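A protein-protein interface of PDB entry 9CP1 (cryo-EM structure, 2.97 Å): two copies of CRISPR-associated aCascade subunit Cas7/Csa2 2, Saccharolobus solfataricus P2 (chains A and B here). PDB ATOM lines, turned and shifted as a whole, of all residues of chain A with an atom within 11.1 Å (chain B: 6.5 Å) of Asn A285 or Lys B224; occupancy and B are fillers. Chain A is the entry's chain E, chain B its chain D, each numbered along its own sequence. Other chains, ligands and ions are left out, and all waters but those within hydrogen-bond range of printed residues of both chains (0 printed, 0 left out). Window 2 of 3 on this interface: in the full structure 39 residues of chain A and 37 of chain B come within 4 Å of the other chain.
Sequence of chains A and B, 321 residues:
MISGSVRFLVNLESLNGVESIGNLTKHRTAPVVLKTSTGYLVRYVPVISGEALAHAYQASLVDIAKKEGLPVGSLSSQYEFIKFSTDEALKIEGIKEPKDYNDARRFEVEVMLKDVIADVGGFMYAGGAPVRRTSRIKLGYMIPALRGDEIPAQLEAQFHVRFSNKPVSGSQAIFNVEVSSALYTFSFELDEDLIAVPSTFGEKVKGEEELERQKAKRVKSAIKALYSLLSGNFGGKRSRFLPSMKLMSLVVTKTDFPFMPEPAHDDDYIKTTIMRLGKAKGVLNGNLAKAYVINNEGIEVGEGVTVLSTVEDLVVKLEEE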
ATOM      1  N   THR A 255      23.381 -24.498  26.748  1.00  0.00           N
ATOM      2  CA  THR A 255      23.860 -23.283  26.103  1.00  0.00           C
ATOM      3  C   THR A 255      25.357 -23.378  25.857  1.00  0.00           C
ATOM      4  O   THR A 255      26.033 -24.292  26.335  1.00  0.00           O
ATOM      5  CB  THR A 255      23.578 -22.028  26.942  1.00  0.00           C
ATOM      6  OG1 THR A 255      24.413 -22.034  28.105  1.00  0.00           O
ATOM      7  CG2 THR A 255      22.122 -21.966  27.367  1.00  0.00           C
ATOM      8  N   ASP A 256      25.865 -22.411  25.093  1.00  0.00           N
ATOM      9  CA  ASP A 256      27.293 -22.230  24.873  1.00  0.00           C
ATOM     10  C   ASP A 256      27.868 -21.076  25.681  1.00  0.00           C
ATOM     11  O   ASP A 256      29.067 -20.801  25.581  1.00  0.00           O
ATOM     12  CB  ASP A 256      27.573 -21.997  23.386  1.00  0.00           C
ATOM     13  CG  ASP A 256      27.285 -23.218  22.544  1.00  0.00           C
ATOM     14  OD1 ASP A 256      26.767 -24.211  23.096  1.00  0.00           O
ATOM     15  OD2 ASP A 256      27.575 -23.186  21.330  1.00  0.00           O
ATOM     16  N   PHE A 257      27.045 -20.399  26.468  1.00  0.00           N
ATOM     17  CA  PHE A 257      27.416 -19.226  27.241  1.00  0.00           C
ATOM     18  C   PHE A 257      26.860 -19.363  28.648  1.00  0.00           C
ATOM     19  O   PHE A 257      25.916 -20.125  28.877  1.00  0.00           O
ATOM     20  CB  PHE A 257      26.880 -17.945  26.581  1.00  0.00           C
ATOM     21  CG  PHE A 257      25.421 -18.007  26.235  1.00  0.00           C
ATOM     22  CD1 PHE A 257      25.009 -18.498  25.009  1.00  0.00           C
ATOM     23  CD2 PHE A 257      24.462 -17.585  27.136  1.00  0.00           C
ATOM     24  CE1 PHE A 257      23.670 -18.560  24.686  1.00  0.00           C
ATOM     25  CE2 PHE A 257      23.120 -17.647  26.820  1.00  0.00           C
ATOM     26  CZ  PHE A 257      22.724 -18.135  25.593  1.00  0.00           C
ATOM     27  N   PRO A 258      27.433 -18.650  29.619  1.00  0.00           N
ATOM     28  CA  PRO A 258      26.922 -18.739  30.993  1.00  0.00           C
ATOM     29  C   PRO A 258      25.456 -18.339  31.079  1.00  0.00           C
ATOM     30  O   PRO A 258      25.017 -17.375  30.450  1.00  0.00           O
ATOM     31  CB  PRO A 258      27.815 -17.763  31.767  1.00  0.00           C
ATOM     32  CG  PRO A 258      29.059 -17.662  30.960  1.00  0.00           C
ATOM     33  CD  PRO A 258      28.643 -17.813  29.532  1.00  0.00           C
ATOM     34  N   ARG A 276      14.228 -15.035  28.996  1.00  0.00           N
ATOM     35  CA  ARG A 276      15.573 -14.593  29.332  1.00  0.00           C
ATOM     36  C   ARG A 276      16.616 -15.336  28.511  1.00  0.00           C
ATOM     37  O   ARG A 276      17.634 -14.756  28.129  1.00  0.00           O
ATOM     38  CB  ARG A 276      15.832 -14.781  30.825  1.00  0.00           C
ATOM     39  CG  ARG A 276      15.570 -13.540  31.654  1.00  0.00           C
ATOM     40  CD  ARG A 276      15.733 -13.832  33.131  1.00  0.00           C
ATOM     41  NE  ARG A 276      17.135 -13.998  33.490  1.00  0.00           N
ATOM     42  CZ  ARG A 276      17.655 -15.118  33.971  1.00  0.00           C
ATOM     43  NH1 ARG A 276      16.914 -16.196  34.162  1.00  0.00           N
ATOM     44  NH2 ARG A 276      18.951 -15.158  34.262  1.00  0.00           N
ATOM     45  N   LEU A 277      16.387 -16.620  28.234  1.00  0.00           N
ATOM     46  CA  LEU A 277      17.328 -17.386  27.425  1.00  0.00           C
ATOM     47  C   LEU A 277      17.406 -16.833  26.012  1.00  0.00           C
ATOM     48  O   LEU A 277      18.497 -16.666  25.455  1.00  0.00           O
ATOM     49  CB  LEU A 277      16.920 -18.858  27.407  1.00  0.00           C
ATOM     50  CG  LEU A 277      17.650 -19.743  26.399  1.00  0.00           C
ATOM     51  CD1 LEU A 277      19.101 -19.908  26.797  1.00  0.00           C
ATOM     52  CD2 LEU A 277      16.968 -21.092  26.296  1.00  0.00           C
ATOM     53  N   GLY A 278      16.251 -16.535  25.417  1.00  0.00           N
ATOM     54  CA  GLY A 278      16.258 -15.943  24.089  1.00  0.00           C
ATOM     55  C   GLY A 278      16.986 -14.611  24.058  1.00  0.00           C
ATOM     56  O   GLY A 278      17.857 -14.377  23.211  1.00  0.00           O
ATOM     57  N   LYS A 279      16.661 -13.730  25.007  1.00  0.00           N
ATOM     58  CA  LYS A 279      17.298 -12.416  25.022  1.00  0.00           C
ATOM     59  C   LYS A 279      18.793 -12.520  25.309  1.00  0.00           C
ATOM     60  O   LYS A 279      19.592 -11.768  24.740  1.00  0.00           O
ATOM     61  CB  LYS A 279      16.605 -11.510  26.035  1.00  0.00           C
ATOM     62  CG  LYS A 279      15.374 -10.818  25.473  1.00  0.00           C
ATOM     63  CD  LYS A 279      14.214 -10.844  26.450  1.00  0.00           C
ATOM     64  CE  LYS A 279      13.015 -10.101  25.888  1.00  0.00           C
ATOM     65  NZ  LYS A 279      12.014  -9.783  26.942  1.00  0.00           N
ATOM     66  N   ALA A 280      19.192 -13.446  26.183  1.00  0.00           N
ATOM     67  CA  ALA A 280      20.604 -13.616  26.500  1.00  0.00           C
ATOM     68  C   ALA A 280      21.379 -14.145  25.304  1.00  0.00           C
ATOM     69  O   ALA A 280      22.499 -13.693  25.036  1.00  0.00           O
ATOM     70  CB  ALA A 280      20.764 -14.550  27.697  1.00  0.00           C
ATOM     71  N   LYS A 281      20.808 -15.109  24.577  1.00  0.00           N
ATOM     72  CA  LYS A 281      21.462 -15.581  23.363  1.00  0.00           C
ATOM     73  C   LYS A 281      21.593 -14.455  22.352  1.00  0.00           C
ATOM     74  O   LYS A 281      22.603 -14.357  21.645  1.00  0.00           O
ATOM     75  CB  LYS A 281      20.694 -16.753  22.757  1.00  0.00           C
ATOM     76  CG  LYS A 281      21.411 -17.387  21.579  1.00  0.00           C
ATOM     77  CD  LYS A 281      20.446 -18.038  20.610  1.00  0.00           C
ATOM     78  CE  LYS A 281      21.180 -18.568  19.392  1.00  0.00           C
ATOM     79  NZ  LYS A 281      20.256 -19.204  18.418  1.00  0.00           N
ATOM     80  N   GLY A 282      20.577 -13.594  22.266  1.00  0.00           N
ATOM     81  CA  GLY A 282      20.683 -12.443  21.386  1.00  0.00           C
ATOM     82  C   GLY A 282      21.790 -11.486  21.790  1.00  0.00           C
ATOM     83  O   GLY A 282      22.534 -10.989  20.942  1.00  0.00           O
ATOM     84  N   VAL A 283      21.921 -11.221  23.089  1.00  0.00           N
ATOM     85  CA  VAL A 283      22.809 -10.154  23.542  1.00  0.00           C
ATOM     86  C   VAL A 283      24.265 -10.603  23.682  1.00  0.00           C
ATOM     87  O   VAL A 283      25.178  -9.797  23.471  1.00  0.00           O
ATOM     88  CB  VAL A 283      22.287  -9.555  24.861  1.00  0.00           C
ATOM     89  CG1 VAL A 283      22.430 -10.541  26.007  1.00  0.00           C
ATOM     90  CG2 VAL A 283      23.010  -8.256  25.181  1.00  0.00           C
ATOM     91  N   LEU A 284      24.516 -11.864  24.027  1.00  0.00           N
ATOM     92  CA  LEU A 284      25.874 -12.321  24.299  1.00  0.00           C
ATOM     93  C   LEU A 284      26.570 -12.913  23.081  1.00  0.00           C
ATOM     94  O   LEU A 284      27.695 -13.403  23.214  1.00  0.00           O
ATOM     95  CB  LEU A 284      25.871 -13.350  25.431  1.00  0.00           C
ATOM     96  CG  LEU A 284      25.988 -12.779  26.843  1.00  0.00           C
ATOM     97  CD1 LEU A 284      25.414 -13.747  27.861  1.00  0.00           C
ATOM     98  CD2 LEU A 284      27.436 -12.455  27.166  1.00  0.00           C
ATOM     99  N   ASN A 285      25.930 -12.886  21.912  1.00  0.00           N
ATOM    100  CA  ASN A 285      26.503 -13.413  20.675  1.00  0.00           C
ATOM    101  C   ASN A 285      26.815 -14.904  20.807  1.00  0.00           C
ATOM    102  O   ASN A 285      27.932 -15.363  20.564  1.00  0.00           O
ATOM    103  CB  ASN A 285      27.752 -12.621  20.268  1.00  0.00           C
ATOM    104  CG  ASN A 285      27.414 -11.306  19.605  1.00  0.00           C
ATOM    105  OD1 ASN A 285      26.514 -11.232  18.770  1.00  0.00           O
ATOM    106  ND2 ASN A 285      28.134 -10.255  19.978  1.00  0.00           N
ATOM    107  N   GLY A 286      25.793 -15.660  21.208  1.00  0.00           N
ATOM    108  CA  GLY A 286      25.906 -17.098  21.311  1.00  0.00           C
ATOM    109  C   GLY A 286      25.634 -17.789  19.988  1.00  0.00           C
ATOM    110  O   GLY A 286      25.372 -17.164  18.961  1.00  0.00           O
ATOM    111  N   ASN A 287      25.705 -19.118  20.025  1.00  0.00           N
ATOM    112  CA  ASN A 287      25.423 -19.917  18.843  1.00  0.00           C
ATOM    113  C   ASN A 287      24.609 -21.170  19.134  1.00  0.00           C
ATOM    114  O   ASN A 287      24.408 -21.974  18.219  1.00  0.00           O
ATOM    115  CB  ASN A 287      26.732 -20.313  18.144  1.00  0.00           C
ATOM    116  CG  ASN A 287      26.553 -20.532  16.659  1.00  0.00           C
ATOM    117  OD1 ASN A 287      25.474 -20.300  16.112  1.00  0.00           O
ATOM    118  ND2 ASN A 287      27.611 -20.980  15.994  1.00  0.00           N
ATOM    119  N   LEU A 288      24.135 -21.363  20.361  1.00  0.00           N
ATOM    120  CA  LEU A 288      23.367 -22.553  20.703  1.00  0.00           C
ATOM    121  C   LEU A 288      22.591 -22.285  21.982  1.00  0.00           C
ATOM    122  O   LEU A 288      23.169 -21.833  22.974  1.00  0.00           O
ATOM    123  CB  LEU A 288      24.283 -23.767  20.880  1.00  0.00           C
ATOM    124  CG  LEU A 288      23.593 -25.085  21.233  1.00  0.00           C
ATOM    125  CD1 LEU A 288      22.654 -25.511  20.117  1.00  0.00           C
ATOM    126  CD2 LEU A 288      24.620 -26.165  21.516  1.00  0.00           C
ATOM    127  N   ALA A 289      21.290 -22.565  21.955  1.00  0.00           N
ATOM    128  CA  ALA A 289      20.454 -22.395  23.140  1.00  0.00           C
ATOM    129  C   ALA A 289      19.240 -23.299  22.989  1.00  0.00           C
ATOM    130  O   ALA A 289      18.384 -23.043  22.138  1.00  0.00           O
ATOM    131  CB  ALA A 289      20.041 -20.940  23.312  1.00  0.00           C
ATOM    132  N   TYR B  57      33.553  -9.121  37.782  1.00  0.00           N
ATOM    133  CA  TYR B  57      33.400  -8.212  36.653  1.00  0.00           C
ATOM    134  C   TYR B  57      34.598  -8.280  35.717  1.00  0.00           C
ATOM    135  O   TYR B  57      34.435  -8.366  34.493  1.00  0.00           O
ATOM    136  CB  TYR B  57      33.200  -6.786  37.165  1.00  0.00           C
ATOM    137  CG  TYR B  57      33.092  -5.740  36.083  1.00  0.00           C
ATOM    138  CD1 TYR B  57      34.221  -5.098  35.600  1.00  0.00           C
ATOM    139  CD2 TYR B  57      31.863  -5.375  35.566  1.00  0.00           C
ATOM    140  CE1 TYR B  57      34.131  -4.141  34.619  1.00  0.00           C
ATOM    141  CE2 TYR B  57      31.763  -4.419  34.583  1.00  0.00           C
ATOM    142  CZ  TYR B  57      32.899  -3.804  34.116  1.00  0.00           C
ATOM    143  OH  TYR B  57      32.805  -2.847  33.136  1.00  0.00           O
ATOM    144  N   ILE B  64      34.821 -11.625  27.485  1.00  0.00           N
ATOM    145  CA  ILE B  64      34.206 -10.940  26.350  1.00  0.00           C
ATOM    146  C   ILE B  64      35.272 -10.346  25.437  1.00  0.00           C
ATOM    147  O   ILE B  64      35.169 -10.425  24.206  1.00  0.00           O
ATOM    148  CB  ILE B  64      33.213  -9.872  26.843  1.00  0.00           C
ATOM    149  CG1 ILE B  64      31.882 -10.525  27.215  1.00  0.00           C
ATOM    150  CG2 ILE B  64      32.987  -8.818  25.780  1.00  0.00           C
ATOM    151  CD1 ILE B  64      30.992  -9.647  28.059  1.00  0.00           C
ATOM    152  N   LYS B  67      36.781 -12.950  23.373  1.00  0.00           N
ATOM    153  CA  LYS B  67      35.823 -13.422  22.380  1.00  0.00           C
ATOM    154  C   LYS B  67      35.720 -12.463  21.199  1.00  0.00           C
ATOM    155  O   LYS B  67      35.566 -12.898  20.052  1.00  0.00           O
ATOM    156  CB  LYS B  67      34.453 -13.629  23.022  1.00  0.00           C
ATOM    157  CG  LYS B  67      33.391 -14.126  22.057  1.00  0.00           C
ATOM    158  CD  LYS B  67      32.182 -14.663  22.796  1.00  0.00           C
ATOM    159  CE  LYS B  67      31.042 -14.956  21.839  1.00  0.00           C
ATOM    160  NZ  LYS B  67      29.897 -15.612  22.525  1.00  0.00           N
ATOM    161  N   GLU B  68      35.806 -11.159  21.452  1.00  0.00           N
ATOM    162  CA  GLU B  68      35.571 -10.167  20.409  1.00  0.00           C
ATOM    163  C   GLU B  68      36.843  -9.690  19.717  1.00  0.00           C
ATOM    164  O   GLU B  68      36.753  -8.874  18.795  1.00  0.00           O
ATOM    165  CB  GLU B  68      34.825  -8.961  20.986  1.00  0.00           C
ATOM    166  CG  GLU B  68      33.318  -9.135  21.020  1.00  0.00           C
ATOM    167  CD  GLU B  68      32.578  -7.816  20.940  1.00  0.00           C
ATOM    168  OE1 GLU B  68      33.220  -6.789  20.637  1.00  0.00           O
ATOM    169  OE2 GLU B  68      31.353  -7.806  21.182  1.00  0.00           O
ATOM    170  N   VAL B 219      34.197   0.551  24.800  1.00  0.00           N
ATOM    171  CA  VAL B 219      33.021   0.993  25.545  1.00  0.00           C
ATOM    172  C   VAL B 219      31.916  -0.051  25.458  1.00  0.00           C
ATOM    173  O   VAL B 219      31.244  -0.353  26.454  1.00  0.00           O
ATOM    174  CB  VAL B 219      32.551   2.366  25.031  1.00  0.00           C
ATOM    175  CG1 VAL B 219      31.199   2.718  25.612  1.00  0.00           C
ATOM    176  CG2 VAL B 219      33.568   3.432  25.383  1.00  0.00           C
ATOM    177  N   LYS B 220      31.715  -0.622  24.269  1.00  0.00           N
ATOM    178  CA  LYS B 220      30.695  -1.653  24.112  1.00  0.00           C
ATOM    179  C   LYS B 220      30.983  -2.850  25.007  1.00  0.00           C
ATOM    180  O   LYS B 220      30.083  -3.361  25.684  1.00  0.00           O
ATOM    181  CB  LYS B 220      30.619  -2.082  22.649  1.00  0.00           C
ATOM    182  CG  LYS B 220      29.309  -2.725  22.251  1.00  0.00           C
ATOM    183  CD  LYS B 220      29.154  -2.747  20.742  1.00  0.00           C
ATOM    184  CE  LYS B 220      28.513  -4.038  20.271  1.00  0.00           C
ATOM    185  NZ  LYS B 220      27.144  -4.203  20.825  1.00  0.00           N
ATOM    186  N   SER B 221      32.239  -3.300  25.037  1.00  0.00           N
ATOM    187  CA  SER B 221      32.597  -4.445  25.866  1.00  0.00           C
ATOM    188  C   SER B 221      32.440  -4.130  27.349  1.00  0.00           C
ATOM    189  O   SER B 221      31.950  -4.965  28.121  1.00  0.00           O
ATOM    190  CB  SER B 221      34.027  -4.883  25.558  1.00  0.00           C
ATOM    191  OG  SER B 221      34.083  -5.589  24.333  1.00  0.00           O
ATOM    192  N   ALA B 222      32.854  -2.932  27.769  1.00  0.00           N
ATOM    193  CA  ALA B 222      32.739  -2.562  29.175  1.00  0.00           C
ATOM    194  C   ALA B 222      31.284  -2.517  29.616  1.00  0.00           C
ATOM    195  O   ALA B 222      30.948  -2.959  30.720  1.00  0.00           O
ATOM    196  CB  ALA B 222      33.417  -1.217  29.425  1.00  0.00           C
ATOM    197  N   ILE B 223      30.403  -1.985  28.767  1.00  0.00           N
ATOM    198  CA  ILE B 223      28.985  -1.958  29.113  1.00  0.00           C
ATOM    199  C   ILE B 223      28.410  -3.370  29.119  1.00  0.00           C
ATOM    200  O   ILE B 223      27.574  -3.710  29.964  1.00  0.00           O
ATOM    201  CB  ILE B 223      28.221  -1.031  28.153  1.00  0.00           C
ATOM    202  CG1 ILE B 223      28.601   0.423  28.418  1.00  0.00           C
ATOM    203  CG2 ILE B 223      26.727  -1.197  28.330  1.00  0.00           C
ATOM    204  CD1 ILE B 223      28.235   1.353  27.295  1.00  0.00           C
ATOM    205  N   LYS B 224      28.853  -4.217  28.185  1.00  0.00           N
ATOM    206  CA  LYS B 224      28.382  -5.599  28.154  1.00  0.00           C
ATOM    207  C   LYS B 224      28.781  -6.362  29.407  1.00  0.00           C
ATOM    208  O   LYS B 224      28.024  -7.218  29.876  1.00  0.00           O
ATOM    209  CB  LYS B 224      28.928  -6.314  26.920  1.00  0.00           C
ATOM    210  CG  LYS B 224      27.873  -6.681  25.900  1.00  0.00           C
ATOM    211  CD  LYS B 224      28.487  -7.379  24.704  1.00  0.00           C
ATOM    212  CE  LYS B 224      27.575  -7.294  23.497  1.00  0.00           C
ATOM    213  NZ  LYS B 224      28.073  -8.126  22.368  1.00  0.00           N
ATOM    214  N   ALA B 225      29.964  -6.078  29.952  1.00  0.00           N
ATOM    215  CA  ALA B 225      30.467  -6.854  31.080  1.00  0.00           C
ATOM    216  C   ALA B 225      29.568  -6.776  32.308  1.00  0.00           C
ATOM    217  O   ALA B 225      29.601  -7.689  33.140  1.00  0.00           O
ATOM    218  CB  ALA B 225      31.878  -6.394  31.445  1.00  0.00           C
ATOM    219  N   LEU B 226      28.756  -5.725  32.439  1.00  0.00           N
ATOM    220  CA  LEU B 226      27.922  -5.555  33.625  1.00  0.00           C
ATOM    221  C   LEU B 226      26.847  -6.621  33.759  1.00  0.00           C
ATOM    222  O   LEU B 226      26.229  -6.719  34.827  1.00  0.00           O
ATOM    223  CB  LEU B 226      27.258  -4.178  33.617  1.00  0.00           C
ATOM    224  CG  LEU B 226      28.143  -2.992  33.990  1.00  0.00           C
ATOM    225  CD1 LEU B 226      27.409  -1.685  33.756  1.00  0.00           C
ATOM    226  CD2 LEU B 226      28.594  -3.100  35.431  1.00  0.00           C
ATOM    227  N   TYR B 227      26.588  -7.394  32.704  1.00  0.00           N
ATOM    228  CA  TYR B 227      25.549  -8.413  32.777  1.00  0.00           C
ATOM    229  C   TYR B 227      25.887  -9.466  33.820  1.00  0.00           C
ATOM    230  O   TYR B 227      24.991 -10.019  34.465  1.00  0.00           O
ATOM    231  CB  TYR B 227      25.345  -9.061  31.411  1.00  0.00           C
ATOM    232  CG  TYR B 227      24.315 -10.162  31.429  1.00  0.00           C
ATOM    233  CD1 TYR B 227      23.000  -9.898  31.780  1.00  0.00           C
ATOM    234  CD2 TYR B 227      24.656 -11.466  31.107  1.00  0.00           C
ATOM    235  CE1 TYR B 227      22.053 -10.900  31.804  1.00  0.00           C
ATOM    236  CE2 TYR B 227      23.714 -12.476  31.128  1.00  0.00           C
ATOM    237  CZ  TYR B 227      22.415 -12.186  31.479  1.00  0.00           C
ATOM    238  OH  TYR B 227      21.470 -13.184  31.504  1.00  0.00           O
ATOM    239  N   SER B 228      27.176  -9.754  34.005  1.00  0.00           N
ATOM    240  CA  SER B 228      27.572 -10.719  35.024  1.00  0.00           C
ATOM    241  C   SER B 228      27.228 -10.222  36.421  1.00  0.00           C
ATOM    242  O   SER B 228      26.647 -10.961  37.223  1.00  0.00           O
ATOM    243  CB  SER B 228      29.065 -11.009  34.920  1.00  0.00           C
ATOM    244  OG  SER B 228      29.819  -9.934  35.448  1.00  0.00           O
ATOM    245  N   VAL B 315      20.469  -4.016  29.240  1.00  0.00           N
ATOM    246  CA  VAL B 315      21.805  -4.023  28.647  1.00  0.00           C
ATOM    247  C   VAL B 315      21.744  -3.594  27.185  1.00  0.00           C
ATOM    248  O   VAL B 315      22.572  -2.800  26.718  1.00  0.00           O
ATOM    249  CB  VAL B 315      22.453  -5.410  28.807  1.00  0.00           C
ATOM    250  CG1 VAL B 315      23.774  -5.467  28.064  1.00  0.00           C
ATOM    251  CG2 VAL B 315      22.658  -5.727  30.276  1.00  0.00           C
ATOM    252  N   GLU B 319      23.464  -0.258  25.556  1.00  0.00           N
ATOM    253  CA  GLU B 319      24.375  -0.328  24.417  1.00  0.00           C
ATOM    254  C   GLU B 319      23.907   0.568  23.279  1.00  0.00           C
ATOM    255  O   GLU B 319      24.714   1.270  22.658  1.00  0.00           O
ATOM    256  CB  GLU B 319      24.503  -1.767  23.920  1.00  0.00           C
ATOM    257  CG  GLU B 319      25.297  -2.687  24.818  1.00  0.00           C
ATOM    258  CD  GLU B 319      25.341  -4.102  24.280  1.00  0.00           C
ATOM    259  OE1 GLU B 319      25.414  -4.266  23.044  1.00  0.00           O
ATOM    260  OE2 GLU B 319      25.291  -5.050  25.089  1.00  0.00           O
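O of Leu A284 is in hydrogen-bond range of NZ of Lys B67 (3.2 Å). The backbone carbonyl oxygen (O) of Asn A285 is in hydrogen-bond range of the side-chain amino group (NZ) of Lys B67 (2.8 Å). ND2 of Asn A285 lies close to NZ of Lys B224 (3.2 Å).
NZ of Lys B224 lies within salt-bridge range of OE2 of Glu B68, at 3.5 Å. NZ of Lys B220 is in salt-bridge range of OE1 of Glu B319, at 2.8 Å.
Among the printed residues, merely in contact across the chains: Val A283 with Lys B224, Val A283 with Glu B319 and Leu A284 with Tyr B227.
Printed residues of chain B within 4 Å of Asn A285: Lys B67 and Lys B224. Of chain A, only Val A283 and Asn A285 come within 4 Å of Lys B224. No residue of chain A comes within 4 Å of Lys B220. No residue of chain A comes within 4 Å of Ser B221. No residue of chain A comes within 4 Å of Ile B223. No residue of chain A comes within 4 Å of Ala B225. Printed residues of chain B within 4 Å of Leu A284: Lys B67 (3.2 Å) and Tyr B227 (3.9 Å). Of the printed residues of chain B, Val A283 touches Lys B224 (3.5 Å) and Glu B319 (3.9 Å). Printed residues of chain A within 4 Å of Glu B319: Val A283. Of the printed residues of chain A, Tyr B227 touches Leu A284. Tyr B57 touches none of the printed residues of chain A. The nearest residue of chain A that does not touch Lys B224 is Leu A284 (5.1 Å). The nearest printed residue of chain A that does not touch Tyr B227 is Ala A280 (4.1 Å).
Of the 16 printed residues of chain B, 4 touch a printed residue of chain A. Of the 18 printed residues of chain A, 3 touch a printed residue of chain B. Hydrophobic or aromatic side chains of chain A that line the printed part of chain B: Val A283 and Leu A284. Among the printed residues, 6 pairs touch across the chains.
No position is printed for both chains.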
